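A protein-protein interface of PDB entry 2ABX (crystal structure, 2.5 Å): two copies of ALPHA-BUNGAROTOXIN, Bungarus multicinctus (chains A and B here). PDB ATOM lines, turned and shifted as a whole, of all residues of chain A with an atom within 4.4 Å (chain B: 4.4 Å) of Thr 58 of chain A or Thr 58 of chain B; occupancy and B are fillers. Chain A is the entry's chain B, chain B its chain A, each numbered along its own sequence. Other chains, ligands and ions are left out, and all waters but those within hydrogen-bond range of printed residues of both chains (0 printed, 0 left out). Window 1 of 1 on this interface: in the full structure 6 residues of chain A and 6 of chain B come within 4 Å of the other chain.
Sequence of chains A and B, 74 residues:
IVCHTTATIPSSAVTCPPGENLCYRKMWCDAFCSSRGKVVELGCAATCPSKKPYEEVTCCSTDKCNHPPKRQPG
OG1 of Thr 58 of chain B lies close to O of Val 57 of chain A (2.8 Å). The side-chain hydroxyl (OG1) of Thr 58 of chain B lies within hydrogen-bond range of the backbone NH (N) of Thr 58 of chain A, at 3.1 Å.
The side-chain amino group (NZ) of Lys 51 of chain B is in hydrogen-bond range of the backbone carbonyl oxygen (O) of Thr 58 of chain B, at 3.2 Å. The backbone carbonyl oxygen (O) of Thr 58 of chain A lies within hydrogen-bond range of the backbone NH (N) of Arg 25 of chain A, at 3.1 Å.
N of Val 57 of chain A touches O of Cys 59 of chain B, at 3.5 Å. Val 57 of chain B touches Cys 59 of chain A.
Printed residues of chain B within 4 Å of Val 57 of chain A: Thr 58 and Cys 59. Of the printed residues of chain B, Cys 59 of chain A touches Val 57 (3.5 Å). Lys 51 of chain B touches none of the printed residues of chain A. Printed residues of chain A within 4 Å of Val 57 of chain B: Cys 59. Of the printed residues of chain A, Thr 58 of chain B touches Val 57 and Thr 58. Of the printed residues of chain A, Cys 59 of chain B touches Val 57. The nearest printed residue of chain A that does not touch Thr 58 of chain B is Cys 59 of chain A (4.9 Å).
Hydrophobic or aromatic side chains of chain A within 4 Å of the printed part of chain B: Val 57. Among the printed residues, 4 pairs touch across the chains. Among the printed residues, no Asp or Glu carboxylate lies within 4 Å of a Lys or Arg side-chain nitrogen of the other chain.
Val 57 of chain A touches Thr 58 of chain B, but with the chains exchanged Thr 58 of chain A does not touch Val 57 of chain B (4.4 Å). Val 57 of chain A touches Cys 59 of chain B, and with the chains exchanged Cys 59 of chain A touches Val 57 of chain B. Thr 58 of chain A touches its own counterpart, Thr 58 of chain B. Of the 4 pairs that touch across the chains among the printed residues, 3 have their exchanged pair printed and touching as well.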
ATOM      1  N   TYR A  24       5.547  -7.089   3.551  1.00  0.00           N
ATOM      2  CA  TYR A  24       4.793  -7.679   2.404  1.00  0.00           C
ATOM      3  C   TYR A  24       3.373  -8.105   2.655  1.00  0.00           C
ATOM      4  O   TYR A  24       2.959  -8.741   3.685  1.00  0.00           O
ATOM      5  CB  TYR A  24       5.778  -8.637   1.709  1.00  0.00           C
ATOM      6  CG  TYR A  24       5.736 -10.065   2.218  1.00  0.00           C
ATOM      7  CD1 TYR A  24       5.043 -11.089   1.518  1.00  0.00           C
ATOM      8  CD2 TYR A  24       6.419 -10.414   3.368  1.00  0.00           C
ATOM      9  CE1 TYR A  24       4.989 -12.371   2.031  1.00  0.00           C
ATOM     10  CE2 TYR A  24       6.398 -11.695   3.897  1.00  0.00           C
ATOM     11  CZ  TYR A  24       5.647 -12.677   3.228  1.00  0.00           C
ATOM     12  OH  TYR A  24       5.714 -13.921   3.749  1.00  0.00           O
ATOM     13  N   ARG A  25       2.480  -7.797   1.674  1.00  0.00           N
ATOM     14  CA  ARG A  25       1.052  -8.017   1.698  1.00  0.00           C
ATOM     15  C   ARG A  25       0.486  -8.927   0.566  1.00  0.00           C
ATOM     16  O   ARG A  25       1.122  -9.056  -0.437  1.00  0.00           O
ATOM     17  CB  ARG A  25       0.209  -6.732   1.715  1.00  0.00           C
ATOM     18  CG  ARG A  25       0.603  -5.571   2.569  1.00  0.00           C
ATOM     19  CD  ARG A  25       0.007  -4.262   2.187  1.00  0.00           C
ATOM     20  NE  ARG A  25      -1.418  -4.126   1.916  1.00  0.00           N
ATOM     21  CZ  ARG A  25      -1.908  -3.962   0.675  1.00  0.00           C
ATOM     22  NH1 ARG A  25      -1.015  -3.867  -0.332  1.00  0.00           N
ATOM     23  NH2 ARG A  25      -3.155  -3.858   0.269  1.00  0.00           N
ATOM     24  N   VAL A  57      -0.896  -8.356  -4.880  1.00  0.00           N
ATOM     25  CA  VAL A  57       0.184  -8.650  -3.849  1.00  0.00           C
ATOM     26  C   VAL A  57       0.901  -7.396  -3.576  1.00  0.00           C
ATOM     27  O   VAL A  57       0.241  -6.286  -3.731  1.00  0.00           O
ATOM     28  CB  VAL A  57       0.415 -10.100  -3.853  1.00  0.00           C
ATOM     29  CG1 VAL A  57       0.525 -10.751  -5.275  1.00  0.00           C
ATOM     30  CG2 VAL A  57       1.344 -10.814  -2.920  1.00  0.00           C
ATOM     31  N   THR A  58       2.105  -7.304  -3.058  1.00  0.00           N
ATOM     32  CA  THR A  58       2.809  -6.059  -2.626  1.00  0.00           C
ATOM     33  C   THR A  58       4.050  -6.392  -1.769  1.00  0.00           C
ATOM     34  O   THR A  58       4.052  -7.364  -0.983  1.00  0.00           O
ATOM     35  CB  THR A  58       1.793  -5.136  -1.900  1.00  0.00           C
ATOM     36  OG1 THR A  58       1.855  -3.864  -2.552  1.00  0.00           O
ATOM     37  CG2 THR A  58       1.930  -5.014  -0.438  1.00  0.00           C
ATOM     38  N   CYS A  59       5.107  -5.660  -2.068  1.00  0.00           N
ATOM     39  CA  CYS A  59       6.479  -5.705  -1.490  1.00  0.00           C
ATOM     40  C   CYS A  59       6.670  -4.188  -1.116  1.00  0.00           C
ATOM     41  O   CYS A  59       7.372  -3.615  -1.880  1.00  0.00           O
ATOM     42  CB  CYS A  59       7.621  -6.174  -2.313  1.00  0.00           C
ATOM     43  SG  CYS A  59       8.446  -7.734  -2.525  1.00  0.00           S
ATOM     44  N   CYS A  60       5.800  -3.772  -0.234  1.00  0.00           N
ATOM     45  CA  CYS A  60       5.777  -2.384   0.311  1.00  0.00           C
ATOM     46  C   CYS A  60       7.196  -2.011   0.749  1.00  0.00           C
ATOM     47  O   CYS A  60       8.193  -2.497   0.226  1.00  0.00           O
ATOM     48  CB  CYS A  60       4.843  -2.525   1.533  1.00  0.00           C
ATOM     49  SG  CYS A  60       5.600  -1.686   3.041  1.00  0.00           S
ATOM     50  N   ARG B  25       3.703  -4.432 -12.223  1.00  0.00           N
ATOM     51  CA  ARG B  25       4.170  -3.097 -11.754  1.00  0.00           C
ATOM     52  C   ARG B  25       5.486  -3.359 -11.005  1.00  0.00           C
ATOM     53  O   ARG B  25       5.530  -4.422 -10.408  1.00  0.00           O
ATOM     54  CB  ARG B  25       3.178  -2.420 -10.835  1.00  0.00           C
ATOM     55  CG  ARG B  25       3.483  -1.157 -10.057  1.00  0.00           C
ATOM     56  CD  ARG B  25       2.563  -0.007 -10.230  1.00  0.00           C
ATOM     57  NE  ARG B  25       2.736   1.090  -9.316  1.00  0.00           N
ATOM     58  CZ  ARG B  25       2.615   2.410  -9.324  1.00  0.00           C
ATOM     59  NH1 ARG B  25       2.178   3.195 -10.255  1.00  0.00           N
ATOM     60  NH2 ARG B  25       3.244   3.080  -8.298  1.00  0.00           N
ATOM     61  N   LYS B  51       9.325 -10.896  -8.936  1.00  0.00           N
ATOM     62  CA  LYS B  51      10.558 -10.152  -9.233  1.00  0.00           C
ATOM     63  C   LYS B  51      11.531 -10.072  -8.080  1.00  0.00           C
ATOM     64  O   LYS B  51      11.751 -11.064  -7.301  1.00  0.00           O
ATOM     65  CB  LYS B  51      10.259  -8.905  -9.966  1.00  0.00           C
ATOM     66  CG  LYS B  51       9.439  -9.141 -11.271  1.00  0.00           C
ATOM     67  CD  LYS B  51       8.959  -7.968 -11.969  1.00  0.00           C
ATOM     68  CE  LYS B  51       7.570  -7.895 -12.571  1.00  0.00           C
ATOM     69  NZ  LYS B  51       6.599  -7.714 -11.393  1.00  0.00           N
ATOM     70  N   VAL B  57       7.499  -2.889  -5.335  1.00  0.00           N
ATOM     71  CA  VAL B  57       6.987  -3.798  -6.391  1.00  0.00           C
ATOM     72  C   VAL B  57       5.491  -4.103  -6.347  1.00  0.00           C
ATOM     73  O   VAL B  57       4.698  -3.313  -5.833  1.00  0.00           O
ATOM     74  CB  VAL B  57       7.895  -5.026  -6.500  1.00  0.00           C
ATOM     75  CG1 VAL B  57       8.234  -5.347  -7.953  1.00  0.00           C
ATOM     76  CG2 VAL B  57       9.165  -4.929  -5.659  1.00  0.00           C
ATOM     77  N   THR B  58       5.084  -5.184  -6.999  1.00  0.00           N
ATOM     78  CA  THR B  58       3.858  -5.880  -7.046  1.00  0.00           C
ATOM     79  C   THR B  58       3.516  -6.659  -8.315  1.00  0.00           C
ATOM     80  O   THR B  58       4.406  -6.977  -9.129  1.00  0.00           O
ATOM     81  CB  THR B  58       2.618  -5.453  -6.247  1.00  0.00           C
ATOM     82  OG1 THR B  58       1.722  -6.574  -6.098  1.00  0.00           O
ATOM     83  CG2 THR B  58       1.810  -4.275  -6.724  1.00  0.00           C
ATOM     84  N   CYS B  59       2.236  -6.911  -8.327  1.00  0.00           N
ATOM     85  CA  CYS B  59       1.340  -7.698  -9.163  1.00  0.00           C
ATOM     86  C   CYS B  59      -0.180  -7.338  -9.009  1.00  0.00           C
ATOM     87  O   CYS B  59      -0.936  -8.118  -8.380  1.00  0.00           O
ATOM     88  CB  CYS B  59       1.584  -9.128  -8.648  1.00  0.00           C
ATOM     89  SG  CYS B  59       1.738 -10.676  -8.936  1.00  0.00           S
ATOM     90  N   CYS B  60      -0.692  -6.283  -9.685  1.00  0.00           N
ATOM     91  CA  CYS B  60      -2.081  -5.806  -9.744  1.00  0.00           C
ATOM     92  C   CYS B  60      -3.004  -6.861 -10.360  1.00  0.00           C
ATOM     93  O   CYS B  60      -2.791  -7.974  -9.825  1.00  0.00           O
ATOM     94  CB  CYS B  60      -2.286  -4.478 -10.477  1.00  0.00           C
ATOM     95  SG  CYS B  60      -2.965  -3.135  -9.397  1.00  0.00           S
